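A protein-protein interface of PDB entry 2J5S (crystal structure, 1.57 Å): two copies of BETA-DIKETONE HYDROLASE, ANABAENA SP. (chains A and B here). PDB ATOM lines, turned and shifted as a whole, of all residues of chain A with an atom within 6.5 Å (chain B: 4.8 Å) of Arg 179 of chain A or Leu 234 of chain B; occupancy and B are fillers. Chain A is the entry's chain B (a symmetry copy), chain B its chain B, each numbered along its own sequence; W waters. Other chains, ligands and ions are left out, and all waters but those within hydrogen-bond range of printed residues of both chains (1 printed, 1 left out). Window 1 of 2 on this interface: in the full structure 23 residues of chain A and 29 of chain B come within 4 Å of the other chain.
Water W1 lies within hydrogen-bond range of the side-chain amide oxygen (OE1) of Gln 236 of chain B (2.9 Å), the backbone carbonyl oxygen (O) of Ala 233 of chain B (3.0 Å) and a ring nitrogen (ND1) of His 166 of chain A (3.1 Å).
Of the printed residues of chain B, Arg 179 of chain A touches Leu 136, Thr 137, Thr 138, Asp 139, Arg 231, Leu 234, Thr 235 and Leu 238.
Of the printed residues of chain A, Leu 234 of chain B touches His 166, Leu 175, Arg 179 and Phe 183.
Of the printed residues of chain A, Thr 235 of chain B touches Arg 179 (3.96 Å).
Of the printed residues of chain B, Pro 161 of chain A touches Thr 230 (3.3 Å).
Of the printed residues of chain A, Asp 139 of chain B touches Tyr 176, Arg 179, Tyr 180 and Phe 183.
Printed residues of chain B within 4 Å of Tyr 180 of chain A: Asp 139 (3.3 Å).
Of the printed residues of chain B, Val 160 of chain A touches Thr 230 and Ala 233.
Phe 181 of chain A touches none of the printed residues of chain B.
Val 232 of chain B touches none of the printed residues of chain A.
The nearest printed residue of chain B that does not touch Arg 179 of chain A is Thr 230 of chain B (6.8 Å).
The nearest printed residue of chain B that does not touch Tyr 180 of chain A is Leu 234 of chain B (6.1 Å).
The guanidinium group (NH1) of Arg 231 of chain B lies within hydrogen-bond range of the backbone carbonyl oxygen (O) of Thr 137 of chain B (3.2 Å).
O of Arg 231 of chain B lies within hydrogen-bond range of OG1 of Thr 235 of chain B, 2.8 Å away.
The backbone carbonyl oxygen of Val 232 of chain B sits at hydrogen-bond distance from the side-chain hydroxyl of Thr 235 of chain B (3.4 Å).
O of Pro 170 of chain A is in hydrogen-bond range of N of Leu 175 of chain A, at 3.4 Å.
O of Leu 175 of chain A lies within hydrogen-bond range of NE of Arg 179 of chain A (2.6 Å).
The backbone carbonyl oxygen (O) of Tyr 180 of chain A sits at hydrogen-bond distance from the side-chain hydroxyl (OG1) of Thr 184 of chain A.
Among the printed residues, merely in contact across the chains: Val 160 of chain A with Thr 230 of chain B, Val 160 of chain A with Ala 233 of chain B, Pro 161 of chain A with Thr 230 of chain B, His 166 of chain A with Ala 233 of chain B, His 166 of chain A with Leu 234 of chain B, Leu 175 of chain A with Leu 234 of chain B, Tyr 176 of chain A with Asp 139 of chain B, Tyr 176 of chain A with Leu 238 of chain B, Arg 179 of chain A with Leu 136 of chain B, Arg 179 of chain A with Arg 231 of chain B, Arg 179 of chain A with Leu 234 of chain B, Arg 179 of chain A with Thr 235 of chain B, Arg 179 of chain A with Leu 238 of chain B, Phe 183 of chain A with Asp 139 of chain B, Phe 183 of chain A with Thr 230 of chain B, Phe 183 of chain A with Arg 231 of chain B and Phe 183 of chain A with Leu 234 of chain B.
OH of Tyr 176 of chain A sits at hydrogen-bond distance from O of Leu 136 of chain B (2.7 Å).
O of Thr 137 of chain B is in hydrogen-bond range of NH1 of Arg 179 of chain A, 3.1 Å away.
The backbone carbonyl oxygen (O) of Thr 138 of chain B sits at hydrogen-bond distance from the guanidinium group (NH2) of Arg 179 of chain A, 2.8 Å away.
OD2 of Asp 139 of chain B is in salt-bridge range of NH1 of Arg 179 of chain A, 2.8 Å away.
The backbone NH of Tyr 180 of chain A is in hydrogen-bond range of the backbone carbonyl oxygen of Asp 139 of chain B (3.3 Å).
No position is printed for both chains.
Of the 22 pairs that touch across the chains among the printed residues, none has its exchanged pair printed and touching as well.
Of the 19 printed residues of chain A, 8 touch a printed residue of chain B.
Printed residues of chain A that touch a printed residue of chain B: Val 160, Pro 161, His 166, Leu 175, Tyr 176, Arg 179, Tyr 180 and Phe 183.
Among the printed residues, 22 pairs touch across the chains.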
ATOM      1  N   VAL A 160      -8.472   5.128 -32.338  1.00  0.00           N
ATOM      2  CA  VAL A 160      -7.229   4.521 -31.826  1.00  0.00           C
ATOM      3  C   VAL A 160      -6.158   4.598 -32.901  1.00  0.00           C
ATOM      4  O   VAL A 160      -6.443   4.315 -34.074  1.00  0.00           O
ATOM      5  CB  VAL A 160      -7.451   3.009 -31.500  1.00  0.00           C
ATOM      6  CG1 VAL A 160      -6.147   2.315 -30.931  1.00  0.00           C
ATOM      7  CG2 VAL A 160      -8.575   2.839 -30.478  1.00  0.00           C
ATOM      8  N   PRO A 161      -4.916   4.946 -32.511  1.00  0.00           N
ATOM      9  CA  PRO A 161      -3.757   4.817 -33.423  1.00  0.00           C
ATOM     10  C   PRO A 161      -3.400   3.326 -33.566  1.00  0.00           C
ATOM     11  O   PRO A 161      -2.375   2.870 -33.019  1.00  0.00           O
ATOM     12  CB  PRO A 161      -2.669   5.617 -32.699  1.00  0.00           C
ATOM     13  CG  PRO A 161      -3.007   5.507 -31.238  1.00  0.00           C
ATOM     14  CD  PRO A 161      -4.526   5.522 -31.210  1.00  0.00           C
ATOM     15  N   VAL A 165       1.041   1.868 -36.069  1.00  0.00           N
ATOM     16  CA  VAL A 165       1.809   2.876 -35.305  1.00  0.00           C
ATOM     17  C   VAL A 165       1.935   2.497 -33.843  1.00  0.00           C
ATOM     18  O   VAL A 165       2.965   2.784 -33.202  1.00  0.00           O
ATOM     19  CB  VAL A 165       1.294   4.328 -35.454  1.00  0.00           C
ATOM     20  CG1 VAL A 165       1.531   4.819 -36.900  1.00  0.00           C
ATOM     21  CG2 VAL A 165      -0.154   4.427 -35.068  1.00  0.00           C
ATOM     22  N   HIS A 166       0.897   1.823 -33.332  1.00  0.00           N
ATOM     23  CA  HIS A 166       0.897   1.447 -31.903  1.00  0.00           C
ATOM     24  C   HIS A 166       1.954   0.389 -31.538  1.00  0.00           C
ATOM     25  O   HIS A 166       2.329   0.247 -30.378  1.00  0.00           O
ATOM     26  CB  HIS A 166      -0.470   0.906 -31.474  1.00  0.00           C
ATOM     27  CG  HIS A 166      -0.919  -0.288 -32.262  1.00  0.00           C
ATOM     28  ND1 HIS A 166      -1.291  -1.497 -31.691  1.00  0.00           N
ATOM     29  CD2 HIS A 166      -1.049  -0.447 -33.597  1.00  0.00           C
ATOM     30  CE1 HIS A 166      -1.645  -2.339 -32.652  1.00  0.00           C
ATOM     31  NE2 HIS A 166      -1.505  -1.726 -33.816  1.00  0.00           N
ATOM     32  N   ILE A 167       2.424  -0.339 -32.557  1.00  0.00           N
ATOM     33  CA  ILE A 167       3.442  -1.359 -32.393  1.00  0.00           C
ATOM     34  C   ILE A 167       4.808  -0.813 -32.762  1.00  0.00           C
ATOM     35  O   ILE A 167       5.791  -0.980 -32.022  1.00  0.00           O
ATOM     36  CB  ILE A 167       3.165  -2.565 -33.331  1.00  0.00           C
ATOM     37  CG1 ILE A 167       1.795  -3.181 -33.029  1.00  0.00           C
ATOM     38  CG2 ILE A 167       4.281  -3.614 -33.129  1.00  0.00           C
ATOM     39  CD1 ILE A 167       1.316  -4.151 -34.144  1.00  0.00           C
ATOM     40  N   TRP A 169       5.985   2.492 -33.504  1.00  0.00           N
ATOM     41  CA  TRP A 169       6.591   3.645 -32.828  1.00  0.00           C
ATOM     42  C   TRP A 169       7.190   3.272 -31.461  1.00  0.00           C
ATOM     43  O   TRP A 169       8.275   3.728 -31.142  1.00  0.00           O
ATOM     44  CB  TRP A 169       5.651   4.881 -32.824  1.00  0.00           C
ATOM     45  CG  TRP A 169       5.734   5.629 -34.132  1.00  0.00           C
ATOM     46  CD1 TRP A 169       4.812   5.650 -35.130  1.00  0.00           C
ATOM     47  CD2 TRP A 169       6.834   6.442 -34.584  1.00  0.00           C
ATOM     48  NE1 TRP A 169       5.269   6.402 -36.197  1.00  0.00           N
ATOM     49  CE2 TRP A 169       6.495   6.920 -35.877  1.00  0.00           C
ATOM     50  CE3 TRP A 169       8.069   6.808 -34.021  1.00  0.00           C
ATOM     51  CZ2 TRP A 169       7.348   7.759 -36.628  1.00  0.00           C
ATOM     52  CZ3 TRP A 169       8.918   7.659 -34.767  1.00  0.00           C
ATOM     53  CH2 TRP A 169       8.549   8.109 -36.062  1.00  0.00           C
ATOM     54  N   PRO A 170       6.462   2.488 -30.630  1.00  0.00           N
ATOM     55  CA  PRO A 170       7.092   2.002 -29.399  1.00  0.00           C
ATOM     56  C   PRO A 170       8.275   1.065 -29.651  1.00  0.00           C
ATOM     57  O   PRO A 170       9.179   0.964 -28.803  1.00  0.00           O
ATOM     58  CB  PRO A 170       5.930   1.313 -28.651  1.00  0.00           C
ATOM     59  CG  PRO A 170       4.689   2.098 -29.138  1.00  0.00           C
ATOM     60  CD  PRO A 170       5.007   2.240 -30.633  1.00  0.00           C
ATOM     61  N   LEU A 173      11.020   3.953 -30.688  1.00  0.00           N
ATOM     62  CA  LEU A 173      11.400   4.890 -29.646  1.00  0.00           C
ATOM     63  C   LEU A 173      11.486   4.249 -28.264  1.00  0.00           C
ATOM     64  O   LEU A 173      11.837   4.931 -27.287  1.00  0.00           O
ATOM     65  CB  LEU A 173      10.401   6.041 -29.595  1.00  0.00           C
ATOM     66  CG  LEU A 173      10.213   6.807 -30.895  1.00  0.00           C
ATOM     67  CD1 LEU A 173       9.134   7.888 -30.758  1.00  0.00           C
ATOM     68  CD2 LEU A 173      11.544   7.426 -31.321  1.00  0.00           C
ATOM     69  N   GLY A 174      11.190   2.955 -28.192  1.00  0.00           N
ATOM     70  CA  GLY A 174      11.084   2.280 -26.894  1.00  0.00           C
ATOM     71  C   GLY A 174       9.663   2.436 -26.372  1.00  0.00           C
ATOM     72  O   GLY A 174       8.899   3.332 -26.809  1.00  0.00           O
ATOM     73  N   LEU A 175       9.303   1.556 -25.438  1.00  0.00           N
ATOM     74  CA  LEU A 175       7.931   1.492 -24.927  1.00  0.00           C
ATOM     75  C   LEU A 175       7.561   2.628 -23.951  1.00  0.00           C
ATOM     76  O   LEU A 175       6.478   2.597 -23.319  1.00  0.00           O
ATOM     77  CB  LEU A 175       7.634   0.078 -24.356  1.00  0.00           C
ATOM     78  CG  LEU A 175       6.745  -0.706 -25.367  1.00  0.00           C
ATOM     79  CD1 LEU A 175       6.773  -2.186 -25.081  1.00  0.00           C
ATOM     80  CD2 LEU A 175       5.308  -0.181 -25.275  1.00  0.00           C
ATOM     81  N   TYR A 176       8.436   3.632 -23.832  1.00  0.00           N
ATOM     82  CA  TYR A 176       8.169   4.771 -22.919  1.00  0.00           C
ATOM     83  C   TYR A 176       7.981   6.010 -23.810  1.00  0.00           C
ATOM     84  O   TYR A 176       6.848   6.520 -23.949  1.00  0.00           O
ATOM     85  CB  TYR A 176       9.288   4.898 -21.834  1.00  0.00           C
ATOM     86  CG  TYR A 176       9.195   3.599 -21.099  1.00  0.00           C
ATOM     87  CD1 TYR A 176      10.055   2.542 -21.410  1.00  0.00           C
ATOM     88  CD2 TYR A 176       8.093   3.364 -20.266  1.00  0.00           C
ATOM     89  CE1 TYR A 176       9.869   1.274 -20.835  1.00  0.00           C
ATOM     90  CE2 TYR A 176       7.871   2.111 -19.683  1.00  0.00           C
ATOM     91  CZ  TYR A 176       8.757   1.068 -19.973  1.00  0.00           C
ATOM     92  OH  TYR A 176       8.496  -0.169 -19.425  1.00  0.00           O
ATOM     93  N   ARG A 177       9.048   6.439 -24.464  1.00  0.00           N
ATOM     94  CA  ARG A 177       8.933   7.571 -25.387  1.00  0.00           C
ATOM     95  C   ARG A 177       7.942   7.269 -26.510  1.00  0.00           C
ATOM     96  O   ARG A 177       7.267   8.173 -27.004  1.00  0.00           O
ATOM     97  CB  ARG A 177      10.309   7.923 -25.973  1.00  0.00           C
ATOM     98  CG  ARG A 177      10.270   9.058 -26.991  1.00  0.00           C
ATOM     99  CD  ARG A 177       9.930  10.407 -26.336  1.00  0.00           C
ATOM    100  NE  ARG A 177      10.110  11.521 -27.305  1.00  0.00           N
ATOM    101  CZ  ARG A 177      11.270  12.139 -27.564  1.00  0.00           C
ATOM    102  NH1 ARG A 177      12.415  11.726 -27.018  1.00  0.00           N
ATOM    103  NH2 ARG A 177      11.315  13.171 -28.423  1.00  0.00           N
ATOM    104  N   GLY A 178       7.856   5.992 -26.934  1.00  0.00           N
ATOM    105  CA  GLY A 178       6.901   5.634 -27.992  1.00  0.00           C
ATOM    106  C   GLY A 178       5.449   5.911 -27.589  1.00  0.00           C
ATOM    107  O   GLY A 178       4.628   6.351 -28.392  1.00  0.00           O
ATOM    108  N   ARG A 179       5.101   5.604 -26.337  1.00  0.00           N
ATOM    109  CA  ARG A 179       3.729   5.893 -25.860  1.00  0.00           C
ATOM    110  C   ARG A 179       3.490   7.393 -25.637  1.00  0.00           C
ATOM    111  O   ARG A 179       2.410   7.894 -26.004  1.00  0.00           O
ATOM    112  CB  ARG A 179       3.395   5.075 -24.611  1.00  0.00           C
ATOM    113  CG  ARG A 179       3.291   3.602 -24.935  1.00  0.00           C
ATOM    114  CD  ARG A 179       2.786   2.820 -23.720  1.00  0.00           C
ATOM    115  NE  ARG A 179       3.898   2.663 -22.761  1.00  0.00           N
ATOM    116  CZ  ARG A 179       3.752   2.336 -21.476  1.00  0.00           C
ATOM    117  NH1 ARG A 179       2.544   2.261 -20.899  1.00  0.00           N
ATOM    118  NH2 ARG A 179       4.845   2.133 -20.745  1.00  0.00           N
ATOM    119  N   TYR A 180       4.484   8.100 -25.090  1.00  0.00           N
ATOM    120  CA  TYR A 180       4.409   9.576 -25.019  1.00  0.00           C
ATOM    121  C   TYR A 180       4.185  10.172 -26.406  1.00  0.00           C
ATOM    122  O   TYR A 180       3.299  10.999 -26.600  1.00  0.00           O
ATOM    123  CB  TYR A 180       5.702  10.100 -24.419  1.00  0.00           C
ATOM    124  CG  TYR A 180       5.791  11.611 -24.331  1.00  0.00           C
ATOM    125  CD1 TYR A 180       5.255  12.312 -23.227  1.00  0.00           C
ATOM    126  CD2 TYR A 180       6.415  12.317 -25.348  1.00  0.00           C
ATOM    127  CE1 TYR A 180       5.376  13.727 -23.143  1.00  0.00           C
ATOM    128  CE2 TYR A 180       6.563  13.687 -25.282  1.00  0.00           C
ATOM    129  CZ  TYR A 180       6.027  14.390 -24.177  1.00  0.00           C
ATOM    130  OH  TYR A 180       6.192  15.762 -24.115  1.00  0.00           O
ATOM    131  N   PHE A 181       4.958   9.728 -27.393  1.00  0.00           N
ATOM    132  CA  PHE A 181       4.858  10.252 -28.768  1.00  0.00           C
ATOM    133  C   PHE A 181       3.462  10.080 -29.332  1.00  0.00           C
ATOM    134  O   PHE A 181       2.928  10.987 -29.975  1.00  0.00           O
ATOM    135  CB  PHE A 181       5.891   9.485 -29.619  1.00  0.00           C
ATOM    136  CG  PHE A 181       5.783   9.704 -31.123  1.00  0.00           C
ATOM    137  CD1 PHE A 181       6.424  10.803 -31.737  1.00  0.00           C
ATOM    138  CD2 PHE A 181       5.073   8.797 -31.924  1.00  0.00           C
ATOM    139  CE1 PHE A 181       6.337  10.997 -33.108  1.00  0.00           C
ATOM    140  CE2 PHE A 181       4.979   8.953 -33.301  1.00  0.00           C
ATOM    141  CZ  PHE A 181       5.620  10.070 -33.905  1.00  0.00           C
ATOM    142  N   LEU A 182       2.861   8.904 -29.117  1.00  0.00           N
ATOM    143  CA  LEU A 182       1.518   8.646 -29.666  1.00  0.00           C
ATOM    144  C   LEU A 182       0.440   9.393 -28.878  1.00  0.00           C
ATOM    145  O   LEU A 182      -0.428  10.026 -29.472  1.00  0.00           O
ATOM    146  CB  LEU A 182       1.236   7.141 -29.710  1.00  0.00           C
ATOM    147  CG  LEU A 182       2.149   6.385 -30.691  1.00  0.00           C
ATOM    148  CD1 LEU A 182       1.870   4.868 -30.570  1.00  0.00           C
ATOM    149  CD2 LEU A 182       1.903   6.870 -32.123  1.00  0.00           C
ATOM    150  N   PHE A 183       0.493   9.324 -27.541  1.00  0.00           N
ATOM    151  CA  PHE A 183      -0.602   9.887 -26.750  1.00  0.00           C
ATOM    152  C   PHE A 183      -0.643  11.410 -26.827  1.00  0.00           C
ATOM    153  O   PHE A 183      -1.728  11.991 -26.681  1.00  0.00           O
ATOM    154  CB  PHE A 183      -0.474   9.496 -25.294  1.00  0.00           C
ATOM    155  CG  PHE A 183      -1.291   8.284 -24.920  1.00  0.00           C
ATOM    156  CD1 PHE A 183      -0.666   7.126 -24.399  1.00  0.00           C
ATOM    157  CD2 PHE A 183      -2.675   8.311 -25.067  1.00  0.00           C
ATOM    158  CE1 PHE A 183      -1.457   6.027 -24.011  1.00  0.00           C
ATOM    159  CE2 PHE A 183      -3.469   7.206 -24.697  1.00  0.00           C
ATOM    160  CZ  PHE A 183      -2.829   6.069 -24.158  1.00  0.00           C
ATOM    161  N   THR A 184       0.514  12.037 -27.016  1.00  0.00           N
ATOM    162  CA  THR A 184       0.576  13.512 -27.093  1.00  0.00           C
ATOM    163  C   THR A 184       0.671  14.020 -28.531  1.00  0.00           C
ATOM    164  O   THR A 184       0.764  15.230 -28.744  1.00  0.00           O
ATOM    165  CB  THR A 184       1.754  14.108 -26.279  1.00  0.00           C
ATOM    166  OG1 THR A 184       3.004  13.775 -26.902  1.00  0.00           O
ATOM    167  CG2 THR A 184       1.699  13.628 -24.808  1.00  0.00           C
ATOM    168  N   LEU B 136       7.354   2.377 -14.807  1.00  0.00           N
ATOM    169  CA  LEU B 136       7.548   1.761 -16.121  1.00  0.00           C
ATOM    170  C   LEU B 136       6.327   0.967 -16.670  1.00  0.00           C
ATOM    171  O   LEU B 136       6.460   0.238 -17.674  1.00  0.00           O
ATOM    172  CB  LEU B 136       8.840   0.934 -16.112  1.00  0.00           C
ATOM    173  CG  LEU B 136      10.084   1.744 -15.704  1.00  0.00           C
ATOM    174  CD1 LEU B 136      11.293   0.798 -15.677  1.00  0.00           C
ATOM    175  CD2 LEU B 136      10.334   2.919 -16.668  1.00  0.00           C
ATOM    176  N   THR B 137       5.169   1.080 -15.991  1.00  0.00           N
ATOM    177  CA  THR B 137       3.929   0.622 -16.571  1.00  0.00           C
ATOM    178  C   THR B 137       3.165   1.783 -17.202  1.00  0.00           C
ATOM    179  O   THR B 137       2.186   1.572 -17.922  1.00  0.00           O
ATOM    180  CB  THR B 137       2.981  -0.024 -15.555  1.00  0.00           C
ATOM    181  OG1 THR B 137       2.557   0.953 -14.605  1.00  0.00           O
ATOM    182  CG2 THR B 137       3.647  -1.215 -14.820  1.00  0.00           C
ATOM    183  N   THR B 138       3.601   3.012 -16.893  1.00  0.00           N
ATOM    184  CA  THR B 138       2.804   4.209 -17.275  1.00  0.00           C
ATOM    185  C   THR B 138       3.167   4.766 -18.653  1.00  0.00           C
ATOM    186  O   THR B 138       4.212   4.437 -19.202  1.00  0.00           O
ATOM    187  CB  THR B 138       2.845   5.287 -16.168  1.00  0.00           C
ATOM    188  OG1 THR B 138       4.156   5.871 -16.115  1.00  0.00           O
ATOM    189  CG2 THR B 138       2.505   4.625 -14.802  1.00  0.00           C
ATOM    190  N   ASP B 139       2.258   5.565 -19.207  1.00  0.00           N
ATOM    191  CA  ASP B 139       2.351   5.973 -20.609  1.00  0.00           C
ATOM    192  C   ASP B 139       3.133   7.255 -20.858  1.00  0.00           C
ATOM    193  O   ASP B 139       3.743   7.434 -21.917  1.00  0.00           O
ATOM    194  CB  ASP B 139       0.944   6.157 -21.138  1.00  0.00           C
ATOM    195  CG  ASP B 139       0.152   4.904 -21.018  1.00  0.00           C
ATOM    196  OD1 ASP B 139      -0.754   4.863 -20.159  1.00  0.00           O
ATOM    197  OD2 ASP B 139       0.463   3.964 -21.804  1.00  0.00           O
ATOM    198  N   THR B 230      -6.917   3.147 -26.770  1.00  0.00           N
ATOM    199  CA  THR B 230      -5.517   3.506 -27.056  1.00  0.00           C
ATOM    200  C   THR B 230      -4.616   2.945 -25.942  1.00  0.00           C
ATOM    201  O   THR B 230      -3.555   2.369 -26.235  1.00  0.00           O
ATOM    202  CB  THR B 230      -5.352   5.027 -27.240  1.00  0.00           C
ATOM    203  OG1 THR B 230      -6.158   5.444 -28.342  1.00  0.00           O
ATOM    204  CG2 THR B 230      -3.937   5.373 -27.563  1.00  0.00           C
ATOM    205  N   ARG B 231      -5.058   3.020 -24.690  1.00  0.00           N
ATOM    206  CA  ARG B 231      -4.300   2.403 -23.602  1.00  0.00           C
ATOM    207  C   ARG B 231      -4.142   0.887 -23.835  1.00  0.00           C
ATOM    208  O   ARG B 231      -3.043   0.324 -23.665  1.00  0.00           O
ATOM    209  CB  ARG B 231      -4.988   2.667 -22.254  1.00  0.00           C
ATOM    210  CG  ARG B 231      -4.439   1.877 -21.083  1.00  0.00           C
ATOM    211  CD  ARG B 231      -3.058   2.294 -20.586  1.00  0.00           C
ATOM    212  NE  ARG B 231      -2.791   1.541 -19.348  1.00  0.00           N
ATOM    213  CZ  ARG B 231      -1.675   1.584 -18.637  1.00  0.00           C
ATOM    214  NH1 ARG B 231      -0.681   2.391 -19.014  1.00  0.00           N
ATOM    215  NH2 ARG B 231      -1.570   0.810 -17.541  1.00  0.00           N
ATOM    216  N   VAL B 232      -5.227   0.241 -24.250  1.00  0.00           N
ATOM    217  CA  VAL B 232      -5.193  -1.221 -24.511  1.00  0.00           C
ATOM    218  C   VAL B 232      -4.203  -1.508 -25.612  1.00  0.00           C
ATOM    219  O   VAL B 232      -3.339  -2.397 -25.488  1.00  0.00           O
ATOM    220  CB  VAL B 232      -6.582  -1.770 -24.899  1.00  0.00           C
ATOM    221  CG1 VAL B 232      -6.485  -3.200 -25.458  1.00  0.00           C
ATOM    222  CG2 VAL B 232      -7.519  -1.730 -23.681  1.00  0.00           C
ATOM    223  N   ALA B 233      -4.309  -0.767 -26.707  1.00  0.00           N
ATOM    224  CA  ALA B 233      -3.459  -1.054 -27.883  1.00  0.00           C
ATOM    225  C   ALA B 233      -1.978  -0.900 -27.542  1.00  0.00           C
ATOM    226  O   ALA B 233      -1.137  -1.695 -27.995  1.00  0.00           O
ATOM    227  CB  ALA B 233      -3.823  -0.124 -29.042  1.00  0.00           C
ATOM    228  N   LEU B 234      -1.672   0.131 -26.739  1.00  0.00           N
ATOM    229  CA  LEU B 234      -0.294   0.498 -26.440  1.00  0.00           C
ATOM    230  C   LEU B 234       0.303  -0.333 -25.305  1.00  0.00           C
ATOM    231  O   LEU B 234       1.500  -0.174 -24.978  1.00  0.00           O
ATOM    232  CB  LEU B 234      -0.224   1.998 -26.093  1.00  0.00           C
ATOM    233  CG  LEU B 234       0.017   2.964 -27.253  1.00  0.00           C
ATOM    234  CD1 LEU B 234      -0.967   2.748 -28.412  1.00  0.00           C
ATOM    235  CD2 LEU B 234      -0.035   4.393 -26.770  1.00  0.00           C
ATOM    236  N   THR B 235      -0.505  -1.207 -24.689  1.00  0.00           N
ATOM    237  CA  THR B 235       0.007  -2.008 -23.546  1.00  0.00           C
ATOM    238  C   THR B 235      -0.024  -3.508 -23.784  1.00  0.00           C
ATOM    239  O   THR B 235       0.389  -4.270 -22.907  1.00  0.00           O
ATOM    240  CB  THR B 235      -0.687  -1.688 -22.204  1.00  0.00           C
ATOM    241  OG1 THR B 235      -2.094  -1.953 -22.324  1.00  0.00           O
ATOM    242  CG2 THR B 235      -0.408  -0.229 -21.779  1.00  0.00           C
ATOM    243  N   GLN B 236      -0.489  -3.940 -24.969  1.00  0.00           N
ATOM    244  CA  GLN B 236      -0.559  -5.378 -25.244  1.00  0.00           C
ATOM    245  C   GLN B 236       0.804  -6.051 -25.111  1.00  0.00           C
ATOM    246  O   GLN B 236       0.950  -7.057 -24.399  1.00  0.00           O
ATOM    247  CB  GLN B 236      -1.108  -5.637 -26.659  1.00  0.00           C
ATOM    248  CG  GLN B 236      -1.132  -7.100 -27.024  1.00  0.00           C
ATOM    249  CD  GLN B 236      -1.480  -7.350 -28.468  1.00  0.00           C
ATOM    250  OE1 GLN B 236      -1.083  -6.585 -29.316  1.00  0.00           O
ATOM    251  NE2 GLN B 236      -2.194  -8.449 -28.754  1.00  0.00           N
ATOM    252  N   LEU B 238       3.577  -4.809 -23.773  1.00  0.00           N
ATOM    253  CA  LEU B 238       4.090  -4.585 -22.455  1.00  0.00           C
ATOM    254  C   LEU B 238       3.551  -5.637 -21.475  1.00  0.00           C
ATOM    255  O   LEU B 238       4.294  -6.247 -20.696  1.00  0.00           O
ATOM    256  CB  LEU B 238       3.691  -3.159 -22.033  1.00  0.00           C
ATOM    257  CG  LEU B 238       4.132  -2.729 -20.655  1.00  0.00           C
ATOM    258  CD1 LEU B 238       5.664  -2.715 -20.547  1.00  0.00           C
ATOM    259  CD2 LEU B 238       3.628  -1.308 -20.415  1.00  0.00           C
HETATM  260  O   HOH W   1      -2.136  -3.887 -29.834  1.00  0.00           O
